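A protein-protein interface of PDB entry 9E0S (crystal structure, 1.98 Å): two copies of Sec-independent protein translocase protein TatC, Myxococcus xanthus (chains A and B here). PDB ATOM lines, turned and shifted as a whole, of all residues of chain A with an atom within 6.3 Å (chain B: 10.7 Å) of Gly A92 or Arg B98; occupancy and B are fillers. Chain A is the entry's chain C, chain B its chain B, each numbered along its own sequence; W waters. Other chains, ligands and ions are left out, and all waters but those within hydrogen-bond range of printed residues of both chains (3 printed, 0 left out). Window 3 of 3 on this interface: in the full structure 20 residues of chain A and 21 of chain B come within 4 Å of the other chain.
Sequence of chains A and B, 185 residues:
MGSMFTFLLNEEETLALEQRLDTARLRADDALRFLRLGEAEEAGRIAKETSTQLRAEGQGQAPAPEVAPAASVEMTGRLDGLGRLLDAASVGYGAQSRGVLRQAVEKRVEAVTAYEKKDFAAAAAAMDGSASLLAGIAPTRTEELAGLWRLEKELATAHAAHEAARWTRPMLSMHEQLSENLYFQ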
ATOM      1  N   LEU A  35      15.676  13.152 -22.841  1.00  0.00           N
ATOM      2  CA  LEU A  35      16.761  12.408 -22.208  1.00  0.00           C
ATOM      3  C   LEU A  35      16.438  12.137 -20.742  1.00  0.00           C
ATOM      4  O   LEU A  35      16.751  11.062 -20.228  1.00  0.00           O
ATOM      5  CB  LEU A  35      18.093  13.156 -22.355  1.00  0.00           C
ATOM      6  CG  LEU A  35      19.377  12.377 -22.017  1.00  0.00           C
ATOM      7  CD1 LEU A  35      19.635  11.275 -23.051  1.00  0.00           C
ATOM      8  CD2 LEU A  35      20.615  13.281 -21.904  1.00  0.00           C
ATOM      9  N   ARG A  36      15.776  13.090 -20.063  1.00  0.00           N
ATOM     10  CA  ARG A  36      15.370  12.893 -18.669  1.00  0.00           C
ATOM     11  C   ARG A  36      14.345  11.776 -18.514  1.00  0.00           C
ATOM     12  O   ARG A  36      14.158  11.259 -17.407  1.00  0.00           O
ATOM     13  CB  ARG A  36      14.798  14.189 -18.085  1.00  0.00           C
ATOM     14  CG  ARG A  36      15.857  15.283 -17.865  1.00  0.00           C
ATOM     15  CD  ARG A  36      15.365  16.393 -16.944  1.00  0.00           C
ATOM     16  NE  ARG A  36      16.427  17.355 -16.633  1.00  0.00           N
ATOM     17  CZ  ARG A  36      16.509  18.046 -15.500  1.00  0.00           C
ATOM     18  NH1 ARG A  36      15.640  17.864 -14.513  1.00  0.00           N
ATOM     19  NH2 ARG A  36      17.475  18.950 -15.361  1.00  0.00           N
ATOM     20  N   LEU A  37      13.680  11.403 -19.597  1.00  0.00           N
ATOM     21  CA  LEU A  37      12.758  10.278 -19.619  1.00  0.00           C
ATOM     22  C   LEU A  37      13.373   9.054 -20.272  1.00  0.00           C
ATOM     23  O   LEU A  37      12.647   8.125 -20.631  1.00  0.00           O
ATOM     24  CB  LEU A  37      11.475  10.670 -20.347  1.00  0.00           C
ATOM     25  CG  LEU A  37      10.758  11.887 -19.784  1.00  0.00           C
ATOM     26  CD1 LEU A  37       9.651  12.363 -20.716  1.00  0.00           C
ATOM     27  CD2 LEU A  37      10.227  11.604 -18.370  1.00  0.00           C
ATOM     28  N   GLY A  38      14.688   9.038 -20.454  1.00  0.00           N
ATOM     29  CA  GLY A  38      15.338   7.886 -21.054  1.00  0.00           C
ATOM     30  C   GLY A  38      15.072   7.686 -22.531  1.00  0.00           C
ATOM     31  O   GLY A  38      15.246   6.576 -23.040  1.00  0.00           O
ATOM     32  N   GLU A  39      14.655   8.726 -23.242  1.00  0.00           N
ATOM     33  CA  GLU A  39      14.366   8.609 -24.674  1.00  0.00           C
ATOM     34  C   GLU A  39      15.509   9.242 -25.465  1.00  0.00           C
ATOM     35  O   GLU A  39      15.382  10.299 -26.090  1.00  0.00           O
ATOM     36  CB  GLU A  39      13.025   9.257 -24.998  1.00  0.00           C
ATOM     37  CG  GLU A  39      11.856   8.585 -24.327  1.00  0.00           C
ATOM     38  CD  GLU A  39      11.680   7.128 -24.746  1.00  0.00           C
ATOM     39  OE1 GLU A  39      11.939   6.800 -25.930  1.00  0.00           O
ATOM     40  OE2 GLU A  39      11.280   6.310 -23.886  1.00  0.00           O
ATOM     41  N   ASP A  87      22.913  17.114 -15.993  1.00  0.00           N
ATOM     42  CA  ASP A  87      21.741  17.064 -15.124  1.00  0.00           C
ATOM     43  C   ASP A  87      20.616  16.262 -15.761  1.00  0.00           C
ATOM     44  O   ASP A  87      19.933  15.494 -15.075  1.00  0.00           O
ATOM     45  CB  ASP A  87      21.258  18.469 -14.793  1.00  0.00           C
ATOM     46  CG  ASP A  87      22.263  19.248 -13.957  1.00  0.00           C
ATOM     47  OD1 ASP A  87      23.184  18.628 -13.371  1.00  0.00           O
ATOM     48  OD2 ASP A  87      22.117  20.483 -13.883  1.00  0.00           O
ATOM     49  N   ALA A  88      20.410  16.427 -17.071  1.00  0.00           N
ATOM     50  CA  ALA A  88      19.386  15.645 -17.761  1.00  0.00           C
ATOM     51  C   ALA A  88      19.723  14.164 -17.732  1.00  0.00           C
ATOM     52  O   ALA A  88      18.864  13.324 -17.439  1.00  0.00           O
ATOM     53  CB  ALA A  88      19.236  16.125 -19.206  1.00  0.00           C
ATOM     54  N   ALA A  89      20.973  13.822 -18.045  1.00  0.00           N
ATOM     55  CA  ALA A  89      21.372  12.418 -18.064  1.00  0.00           C
ATOM     56  C   ALA A  89      21.255  11.794 -16.678  1.00  0.00           C
ATOM     57  O   ALA A  89      20.870  10.622 -16.550  1.00  0.00           O
ATOM     58  CB  ALA A  89      22.797  12.294 -18.621  1.00  0.00           C
ATOM     59  N   SER A  90      21.515  12.573 -15.627  1.00  0.00           N
ATOM     60  CA  SER A  90      21.388  12.041 -14.274  1.00  0.00           C
ATOM     61  C   SER A  90      19.941  11.723 -13.921  1.00  0.00           C
ATOM     62  O   SER A  90      19.677  10.736 -13.227  1.00  0.00           O
ATOM     63  CB  SER A  90      21.973  13.029 -13.268  1.00  0.00           C
ATOM     64  OG  SER A  90      23.337  13.246 -13.562  1.00  0.00           O
ATOM     65  N   VAL A  91      18.986  12.558 -14.343  1.00  0.00           N
ATOM     66  CA  VAL A  91      17.582  12.221 -14.082  1.00  0.00           C
ATOM     67  C   VAL A  91      17.162  11.014 -14.913  1.00  0.00           C
ATOM     68  O   VAL A  91      16.470  10.106 -14.425  1.00  0.00           O
ATOM     69  CB  VAL A  91      16.663  13.429 -14.357  1.00  0.00           C
ATOM     70  CG1 VAL A  91      15.202  12.994 -14.331  1.00  0.00           C
ATOM     71  CG2 VAL A  91      16.891  14.547 -13.329  1.00  0.00           C
ATOM     72  N   GLY A  92      17.561  10.979 -16.185  1.00  0.00           N
ATOM     73  CA  GLY A  92      17.079   9.922 -17.059  1.00  0.00           C
ATOM     74  C   GLY A  92      17.717   8.571 -16.806  1.00  0.00           C
ATOM     75  O   GLY A  92      17.126   7.534 -17.126  1.00  0.00           O
ATOM     76  N   TYR A  93      18.931   8.550 -16.255  1.00  0.00           N
ATOM     77  CA  TYR A  93      19.701   7.314 -16.199  1.00  0.00           C
ATOM     78  C   TYR A  93      20.316   7.048 -14.838  1.00  0.00           C
ATOM     79  O   TYR A  93      21.036   6.056 -14.694  1.00  0.00           O
ATOM     80  CB  TYR A  93      20.802   7.319 -17.286  1.00  0.00           C
ATOM     81  CG  TYR A  93      20.208   7.338 -18.685  1.00  0.00           C
ATOM     82  CD1 TYR A  93      19.914   8.542 -19.311  1.00  0.00           C
ATOM     83  CD2 TYR A  93      19.906   6.151 -19.358  1.00  0.00           C
ATOM     84  CE1 TYR A  93      19.333   8.573 -20.563  1.00  0.00           C
ATOM     85  CE2 TYR A  93      19.319   6.168 -20.631  1.00  0.00           C
ATOM     86  CZ  TYR A  93      19.038   7.396 -21.218  1.00  0.00           C
ATOM     87  OH  TYR A  93      18.473   7.465 -22.470  1.00  0.00           O
ATOM     88  N   GLY A  94      20.052   7.894 -13.839  1.00  0.00           N
ATOM     89  CA  GLY A  94      20.619   7.693 -12.518  1.00  0.00           C
ATOM     90  C   GLY A  94      20.146   6.430 -11.828  1.00  0.00           C
ATOM     91  O   GLY A  94      20.850   5.909 -10.957  1.00  0.00           O
ATOM     92  N   ALA A  95      18.965   5.926 -12.188  1.00  0.00           N
ATOM     93  CA  ALA A  95      18.494   4.686 -11.587  1.00  0.00           C
ATOM     94  C   ALA A  95      19.345   3.490 -11.990  1.00  0.00           C
ATOM     95  O   ALA A  95      19.394   2.511 -11.245  1.00  0.00           O
ATOM     96  CB  ALA A  95      17.041   4.429 -11.965  1.00  0.00           C
ATOM     97  N   GLN A  96      20.033   3.555 -13.127  1.00  0.00           N
ATOM     98  CA  GLN A  96      20.768   2.410 -13.647  1.00  0.00           C
ATOM     99  C   GLN A  96      22.260   2.639 -13.846  1.00  0.00           C
ATOM    100  O   GLN A  96      23.012   1.669 -13.797  1.00  0.00           O
ATOM    101  CB  GLN A  96      20.161   1.956 -14.988  1.00  0.00           C
ATOM    102  CG  GLN A  96      19.698   3.110 -15.883  1.00  0.00           C
ATOM    103  CD  GLN A  96      20.026   2.904 -17.363  1.00  0.00           C
ATOM    104  OE1 GLN A  96      21.083   3.336 -17.848  1.00  0.00           O
ATOM    105  NE2 GLN A  96      19.116   2.254 -18.090  1.00  0.00           N
ATOM    106  N   ARG B  36       7.640  16.903  -7.142  1.00  0.00           N
ATOM    107  CA  ARG B  36       8.854  16.121  -7.370  1.00  0.00           C
ATOM    108  C   ARG B  36       8.992  14.961  -6.387  1.00  0.00           C
ATOM    109  O   ARG B  36       9.793  14.049  -6.628  1.00  0.00           O
ATOM    110  CB  ARG B  36      10.092  17.018  -7.276  1.00  0.00           C
ATOM    111  CG  ARG B  36      10.221  17.978  -8.451  1.00  0.00           C
ATOM    112  CD  ARG B  36      11.648  18.514  -8.587  1.00  0.00           C
ATOM    113  NE  ARG B  36      11.738  19.407  -9.734  1.00  0.00           N
ATOM    114  CZ  ARG B  36      12.813  19.567 -10.491  1.00  0.00           C
ATOM    115  NH1 ARG B  36      13.942  18.922 -10.240  1.00  0.00           N
ATOM    116  NH2 ARG B  36      12.745  20.381 -11.544  1.00  0.00           N
ATOM    117  N   LEU B  86       6.592  20.328 -16.284  1.00  0.00           N
ATOM    118  CA  LEU B  86       7.042  19.062 -16.861  1.00  0.00           C
ATOM    119  C   LEU B  86       8.275  18.527 -16.132  1.00  0.00           C
ATOM    120  O   LEU B  86       8.389  17.317 -15.884  1.00  0.00           O
ATOM    121  CB  LEU B  86       7.342  19.232 -18.356  1.00  0.00           C
ATOM    122  CG  LEU B  86       6.164  19.526 -19.293  1.00  0.00           C
ATOM    123  CD1 LEU B  86       6.613  19.711 -20.738  1.00  0.00           C
ATOM    124  CD2 LEU B  86       5.172  18.405 -19.244  1.00  0.00           C
ATOM    125  N   ASP B  87       9.212  19.412 -15.794  1.00  0.00           N
ATOM    126  CA  ASP B  87      10.437  18.991 -15.113  1.00  0.00           C
ATOM    127  C   ASP B  87      10.130  18.456 -13.720  1.00  0.00           C
ATOM    128  O   ASP B  87      10.726  17.462 -13.289  1.00  0.00           O
ATOM    129  CB  ASP B  87      11.437  20.156 -15.025  1.00  0.00           C
ATOM    130  CG  ASP B  87      11.955  20.615 -16.402  1.00  0.00           C
ATOM    131  OD1 ASP B  87      11.923  19.823 -17.371  1.00  0.00           O
ATOM    132  OD2 ASP B  87      12.402  21.779 -16.514  1.00  0.00           O
ATOM    133  N   ALA B  89       7.131  17.171 -12.745  1.00  0.00           N
ATOM    134  CA  ALA B  89       6.411  15.924 -12.979  1.00  0.00           C
ATOM    135  C   ALA B  89       7.356  14.787 -13.346  1.00  0.00           C
ATOM    136  O   ALA B  89       7.156  13.639 -12.918  1.00  0.00           O
ATOM    137  CB  ALA B  89       5.369  16.127 -14.083  1.00  0.00           C
ATOM    138  N   SER B  90       8.393  15.082 -14.136  1.00  0.00           N
ATOM    139  CA  SER B  90       9.305  14.036 -14.594  1.00  0.00           C
ATOM    140  C   SER B  90      10.122  13.468 -13.442  1.00  0.00           C
ATOM    141  O   SER B  90      10.377  12.259 -13.393  1.00  0.00           O
ATOM    142  CB  SER B  90      10.236  14.566 -15.688  1.00  0.00           C
ATOM    143  OG  SER B  90       9.500  14.917 -16.863  1.00  0.00           O
ATOM    144  N   VAL B  91      10.538  14.313 -12.503  1.00  0.00           N
ATOM    145  CA  VAL B  91      11.252  13.781 -11.346  1.00  0.00           C
ATOM    146  C   VAL B  91      10.306  12.978 -10.460  1.00  0.00           C
ATOM    147  O   VAL B  91      10.639  11.883  -9.999  1.00  0.00           O
ATOM    148  CB  VAL B  91      11.931  14.922 -10.566  1.00  0.00           C
ATOM    149  CG1 VAL B  91      12.442  14.416  -9.217  1.00  0.00           C
ATOM    150  CG2 VAL B  91      13.074  15.531 -11.394  1.00  0.00           C
ATOM    151  N   GLY B  92       9.108  13.508 -10.203  1.00  0.00           N
ATOM    152  CA  GLY B  92       8.230  12.878  -9.236  1.00  0.00           C
ATOM    153  C   GLY B  92       7.602  11.576  -9.702  1.00  0.00           C
ATOM    154  O   GLY B  92       7.247  10.747  -8.857  1.00  0.00           O
ATOM    155  N   TYR B  93       7.474  11.374 -11.026  1.00  0.00           N
ATOM    156  CA  TYR B  93       6.679  10.282 -11.582  1.00  0.00           C
ATOM    157  C   TYR B  93       7.376   9.527 -12.703  1.00  0.00           C
ATOM    158  O   TYR B  93       6.776   8.603 -13.267  1.00  0.00           O
ATOM    159  CB  TYR B  93       5.322  10.811 -12.088  1.00  0.00           C
ATOM    160  CG  TYR B  93       4.494  11.396 -10.974  1.00  0.00           C
ATOM    161  CD1 TYR B  93       4.654  12.732 -10.584  1.00  0.00           C
ATOM    162  CD2 TYR B  93       3.576  10.607 -10.275  1.00  0.00           C
ATOM    163  CE1 TYR B  93       3.920  13.269  -9.534  1.00  0.00           C
ATOM    164  CE2 TYR B  93       2.831  11.140  -9.233  1.00  0.00           C
ATOM    165  CZ  TYR B  93       3.000  12.463  -8.871  1.00  0.00           C
ATOM    166  OH  TYR B  93       2.263  12.991  -7.839  1.00  0.00           O
ATOM    167  N   GLY B  94       8.618   9.881 -13.031  1.00  0.00           N
ATOM    168  CA  GLY B  94       9.360   9.220 -14.090  1.00  0.00           C
ATOM    169  C   GLY B  94       9.694   7.774 -13.791  1.00  0.00           C
ATOM    170  O   GLY B  94       9.987   7.011 -14.717  1.00  0.00           O
ATOM    171  N   ALA B  95       9.656   7.374 -12.522  1.00  0.00           N
ATOM    172  CA  ALA B  95       9.924   5.975 -12.222  1.00  0.00           C
ATOM    173  C   ALA B  95       8.822   5.076 -12.774  1.00  0.00           C
ATOM    174  O   ALA B  95       9.088   3.933 -13.155  1.00  0.00           O
ATOM    175  CB  ALA B  95      10.083   5.775 -10.714  1.00  0.00           C
ATOM    176  N   GLN B  96       7.595   5.582 -12.864  1.00  0.00           N
ATOM    177  CA  GLN B  96       6.445   4.764 -13.225  1.00  0.00           C
ATOM    178  C   GLN B  96       5.707   5.234 -14.468  1.00  0.00           C
ATOM    179  O   GLN B  96       5.118   4.402 -15.160  1.00  0.00           O
ATOM    180  CB  GLN B  96       5.445   4.718 -12.056  1.00  0.00           C
ATOM    181  CG  GLN B  96       6.075   4.448 -10.687  1.00  0.00           C
ATOM    182  CD  GLN B  96       6.512   2.996 -10.503  1.00  0.00           C
ATOM    183  OE1 GLN B  96       6.068   2.101 -11.229  1.00  0.00           O
ATOM    184  NE2 GLN B  96       7.385   2.759  -9.525  1.00  0.00           N
ATOM    185  N   SER B  97       5.724   6.533 -14.775  1.00  0.00           N
ATOM    186  CA  SER B  97       4.818   7.116 -15.758  1.00  0.00           C
ATOM    187  C   SER B  97       5.547   7.692 -16.964  1.00  0.00           C
ATOM    188  O   SER B  97       5.098   8.687 -17.542  1.00  0.00           O
ATOM    189  CB  SER B  97       3.964   8.202 -15.109  1.00  0.00           C
ATOM    190  OG  SER B  97       3.156   7.639 -14.095  1.00  0.00           O
ATOM    191  N   ARG B  98       6.642   7.068 -17.396  1.00  0.00           N
ATOM    192  CA  ARG B  98       7.379   7.647 -18.518  1.00  0.00           C
ATOM    193  C   ARG B  98       6.551   7.679 -19.793  1.00  0.00           C
ATOM    194  O   ARG B  98       6.748   8.567 -20.625  1.00  0.00           O
ATOM    195  CB  ARG B  98       8.682   6.895 -18.754  1.00  0.00           C
ATOM    196  CG  ARG B  98       9.812   7.468 -17.896  1.00  0.00           C
ATOM    197  CD  ARG B  98      11.068   6.639 -17.989  1.00  0.00           C
ATOM    198  NE  ARG B  98      12.153   7.256 -17.242  1.00  0.00           N
ATOM    199  CZ  ARG B  98      13.415   6.868 -17.323  1.00  0.00           C
ATOM    200  NH1 ARG B  98      13.775   5.850 -18.093  1.00  0.00           N
ATOM    201  NH2 ARG B  98      14.337   7.512 -16.614  1.00  0.00           N
ATOM    202  N   GLY B  99       5.620   6.734 -19.964  1.00  0.00           N
ATOM    203  CA  GLY B  99       4.777   6.751 -21.153  1.00  0.00           C
ATOM    204  C   GLY B  99       3.969   8.027 -21.259  1.00  0.00           C
ATOM    205  O   GLY B  99       3.967   8.697 -22.295  1.00  0.00           O
ATOM    206  N   VAL B 100       3.285   8.386 -20.177  1.00  0.00           N
ATOM    207  CA  VAL B 100       2.471   9.591 -20.174  1.00  0.00           C
ATOM    208  C   VAL B 100       3.348  10.840 -20.228  1.00  0.00           C
ATOM    209  O   VAL B 100       3.030  11.804 -20.931  1.00  0.00           O
ATOM    210  CB  VAL B 100       1.555   9.589 -18.941  1.00  0.00           C
ATOM    211  CG1 VAL B 100       0.858  10.908 -18.802  1.00  0.00           C
ATOM    212  CG2 VAL B 100       0.540   8.461 -19.050  1.00  0.00           C
ATOM    213  N   LEU B 101       4.459  10.844 -19.489  1.00  0.00           N
ATOM    214  CA  LEU B 101       5.352  12.006 -19.476  1.00  0.00           C
ATOM    215  C   LEU B 101       5.919  12.285 -20.861  1.00  0.00           C
ATOM    216  O   LEU B 101       6.042  13.448 -21.270  1.00  0.00           O
ATOM    217  CB  LEU B 101       6.475  11.769 -18.470  1.00  0.00           C
ATOM    218  CG  LEU B 101       6.016  11.768 -17.015  1.00  0.00           C
ATOM    219  CD1 LEU B 101       7.048  11.053 -16.120  1.00  0.00           C
ATOM    220  CD2 LEU B 101       5.769  13.187 -16.529  1.00  0.00           C
ATOM    221  N   ARG B 102       6.262  11.230 -21.605  1.00  0.00           N
ATOM    222  CA  ARG B 102       6.734  11.421 -22.972  1.00  0.00           C
ATOM    223  C   ARG B 102       5.676  12.091 -23.843  1.00  0.00           C
ATOM    224  O   ARG B 102       5.998  12.960 -24.660  1.00  0.00           O
ATOM    225  CB  ARG B 102       7.145  10.084 -23.573  1.00  0.00           C
ATOM    226  CG  ARG B 102       8.422   9.513 -22.985  1.00  0.00           C
ATOM    227  CD  ARG B 102       8.496   8.018 -23.277  1.00  0.00           C
ATOM    228  NE  ARG B 102       8.518   7.751 -24.712  1.00  0.00           N
ATOM    229  CZ  ARG B 102       8.114   6.621 -25.277  1.00  0.00           C
ATOM    230  NH1 ARG B 102       7.577   5.642 -24.560  1.00  0.00           N
ATOM    231  NH2 ARG B 102       8.248   6.473 -26.593  1.00  0.00           N
ATOM    232  N   GLN B 103       4.415  11.679 -23.700  1.00  0.00           N
ATOM    233  CA  GLN B 103       3.331  12.340 -24.419  1.00  0.00           C
ATOM    234  C   GLN B 103       3.261  13.813 -24.066  1.00  0.00           C
ATOM    235  O   GLN B 103       3.019  14.656 -24.937  1.00  0.00           O
ATOM    236  CB  GLN B 103       1.995  11.683 -24.088  1.00  0.00           C
ATOM    237  CG  GLN B 103       1.862  10.245 -24.586  1.00  0.00           C
ATOM    238  CD  GLN B 103       0.647   9.561 -23.986  1.00  0.00           C
ATOM    239  OE1 GLN B 103       0.020  10.083 -23.064  1.00  0.00           O
ATOM    240  NE2 GLN B 103       0.306   8.402 -24.508  1.00  0.00           N
ATOM    241  N   ALA B 104       3.387  14.134 -22.777  1.00  0.00           N
ATOM    242  CA  ALA B 104       3.281  15.532 -22.368  1.00  0.00           C
ATOM    243  C   ALA B 104       4.424  16.353 -22.948  1.00  0.00           C
ATOM    244  O   ALA B 104       4.219  17.497 -23.391  1.00  0.00           O
ATOM    245  CB  ALA B 104       3.250  15.636 -20.840  1.00  0.00           C
ATOM    246  N   VAL B 105       5.632  15.783 -22.975  1.00  0.00           N
ATOM    247  CA  VAL B 105       6.763  16.499 -23.564  1.00  0.00           C
ATOM    248  C   VAL B 105       6.589  16.639 -25.076  1.00  0.00           C
ATOM    249  O   VAL B 105       6.909  17.680 -25.652  1.00  0.00           O
ATOM    250  CB  VAL B 105       8.096  15.813 -23.211  1.00  0.00           C
ATOM    251  CG1 VAL B 105       9.266  16.484 -23.984  1.00  0.00           C
ATOM    252  CG2 VAL B 105       8.361  15.918 -21.715  1.00  0.00           C
ATOM    253  N   GLU B 106       6.089  15.598 -25.748  1.00  0.00           N
ATOM    254  CA  GLU B 106       5.817  15.724 -27.179  1.00  0.00           C
ATOM    255  C   GLU B 106       4.866  16.877 -27.464  1.00  0.00           C
ATOM    256  O   GLU B 106       5.043  17.609 -28.445  1.00  0.00           O
ATOM    257  CB  GLU B 106       5.240  14.406 -27.728  1.00  0.00           C
ATOM    258  CG  GLU B 106       6.299  13.314 -27.842  1.00  0.00           C
ATOM    259  CD  GLU B 106       5.725  11.917 -28.036  1.00  0.00           C
ATOM    260  OE1 GLU B 106       4.532  11.807 -28.390  1.00  0.00           O
ATOM    261  OE2 GLU B 106       6.479  10.935 -27.831  1.00  0.00           O
ATOM    262  N   LEU B 133      -2.436  16.083 -20.257  1.00  0.00           N
ATOM    263  CA  LEU B 133      -1.884  14.734 -20.302  1.00  0.00           C
ATOM    264  C   LEU B 133      -1.261  14.337 -18.970  1.00  0.00           C
ATOM    265  O   LEU B 133      -1.278  13.158 -18.609  1.00  0.00           O
ATOM    266  CB  LEU B 133      -0.851  14.629 -21.430  1.00  0.00           C
ATOM    267  CG  LEU B 133      -1.448  14.626 -22.841  1.00  0.00           C
ATOM    268  CD1 LEU B 133      -0.391  14.760 -23.919  1.00  0.00           C
ATOM    269  CD2 LEU B 133      -2.256  13.360 -23.062  1.00  0.00           C
ATOM    270  N   LEU B 134      -0.705  15.301 -18.229  1.00  0.00           N
ATOM    271  CA  LEU B 134      -0.092  14.983 -16.941  1.00  0.00           C
ATOM    272  C   LEU B 134      -1.099  14.463 -15.924  1.00  0.00           C
ATOM    273  O   LEU B 134      -0.689  13.824 -14.954  1.00  0.00           O
ATOM    274  CB  LEU B 134       0.614  16.209 -16.360  1.00  0.00           C
ATOM    275  CG  LEU B 134       1.848  16.720 -17.120  1.00  0.00           C
ATOM    276  CD1 LEU B 134       2.316  18.017 -16.508  1.00  0.00           C
ATOM    277  CD2 LEU B 134       2.995  15.715 -17.135  1.00  0.00           C
ATOM    278  N   GLY B 136      -2.728  11.979 -16.142  1.00  0.00           N
ATOM    279  CA  GLY B 136      -2.531  10.541 -16.135  1.00  0.00           C
ATOM    280  C   GLY B 136      -1.431  10.049 -15.209  1.00  0.00           C
ATOM    281  O   GLY B 136      -1.338   8.838 -14.984  1.00  0.00           O
ATOM    282  N   ILE B 137      -0.593  10.938 -14.677  1.00  0.00           N
ATOM    283  CA  ILE B 137       0.431  10.469 -13.748  1.00  0.00           C
ATOM    284  C   ILE B 137      -0.133  10.306 -12.339  1.00  0.00           C
ATOM    285  O   ILE B 137       0.410   9.530 -11.545  1.00  0.00           O
ATOM    286  CB  ILE B 137       1.658  11.401 -13.731  1.00  0.00           C
ATOM    287  CG1 ILE B 137       1.358  12.682 -12.942  1.00  0.00           C
ATOM    288  CG2 ILE B 137       2.136  11.727 -15.160  1.00  0.00           C
ATOM    289  CD1 ILE B 137       2.436  13.767 -13.124  1.00  0.00           C
ATOM    290  N   ALA B 138      -1.184  11.047 -11.983  1.00  0.00           N
ATOM    291  CA  ALA B 138      -1.797  10.970 -10.655  1.00  0.00           C
ATOM    292  C   ALA B 138      -3.300  11.160 -10.817  1.00  0.00           C
ATOM    293  O   ALA B 138      -3.855  12.220 -10.499  1.00  0.00           O
ATOM    294  CB  ALA B 138      -1.196  12.015  -9.710  1.00  0.00           C
HETATM  295  O   HOH W   1      12.644   9.630 -15.775  1.00  0.00           O
HETATM  296  O   HOH W   2      13.068  16.768 -14.774  1.00  0.00           O
HETATM  297  O   HOH W   3      16.631   5.137 -18.349  1.00  0.00           O
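The guanidinium group (NH2) of Arg B98 is in hydrogen-bond range of the backbone carbonyl oxygen (O) of Gly A92, 2.8 Å away.
OE2 of Glu A39 is in salt-bridge range of NE of Arg B102.
The side-chain hydroxyl (OG) of Ser B90 sits at hydrogen-bond distance from the backbone carbonyl oxygen (O) of Leu B86, at 2.8 Å.
The guanidinium group of Arg B98 sits close to the backbone carbonyl oxygen of Gly B94, at 3.3 Å.
The side-chain hydroxyl (OH) of Tyr A93 sits at hydrogen-bond distance from the backbone carbonyl oxygen (O) of Gly A38, at 3.4 Å.
Among the printed residues, pairs that only touch across the chains: Leu A37 with Arg B98 (3.4 Å), Leu A37 with Arg B102 (3.7 Å), Leu A37 with Ser B90 (3.7 Å), Leu A37 with Leu B101 (3.7 Å), Arg A36 with Arg B98 (3.8 Å), Leu A37 with Val B105 (3.9 Å) and Gly A38 with Arg B98 (3.9 Å).
Of the printed residues of chain B, Arg A36 touches Arg B98.
Of chain B, only Arg B98 comes within 4 Å of Gly A38.
Ala A88 touches none of the printed residues of chain B.
No residue of chain B comes within 4 Å of Ala A89.
Ser A90 touches none of the printed residues of chain B.
Gly A92 touches one residue of chain B.
No residue of chain B comes within 4 Å of Tyr A93.
Printed residues of chain A within 4 Å of Arg B98: Arg A36, Leu A37, Gly A38 and Gly A92.
Of the printed residues of chain A, Val B105 touches Leu A37.
The nearest residue of chain B that does not touch Gly A92 is Gly B94 (7.6 Å).
The nearest printed residue of chain A that does not touch Arg B98 is Val A91 (4.01 Å).
The nearest printed residue of chain A that does not touch Val B105 is Leu A35 (7.3 Å).
Hydrophobic or aromatic side chains of chain B that line the printed part of chain A: Leu B101 and Val B105.
Hydrophobic or aromatic side chains of chain A that line the printed part of chain B: Leu A37.
Positions printed for both chains: 36, 87, 89, 90, 91, 92, 93, 94, 95 and 96.
Of the 9 pairs that touch across the chains among the printed residues, none has its exchanged pair printed and touching as well.
Water W3 bridges O of Gly A92 and NH1 of Arg B98.
Water W1 bridges O of Arg A36 (2.8 Å) and NE of Arg B98 (2.8 Å).
Water W2 bridges the guanidinium group of Arg A36 (2.8 Å) and the backbone carbonyl oxygen of Asp B87 (2.9 Å).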
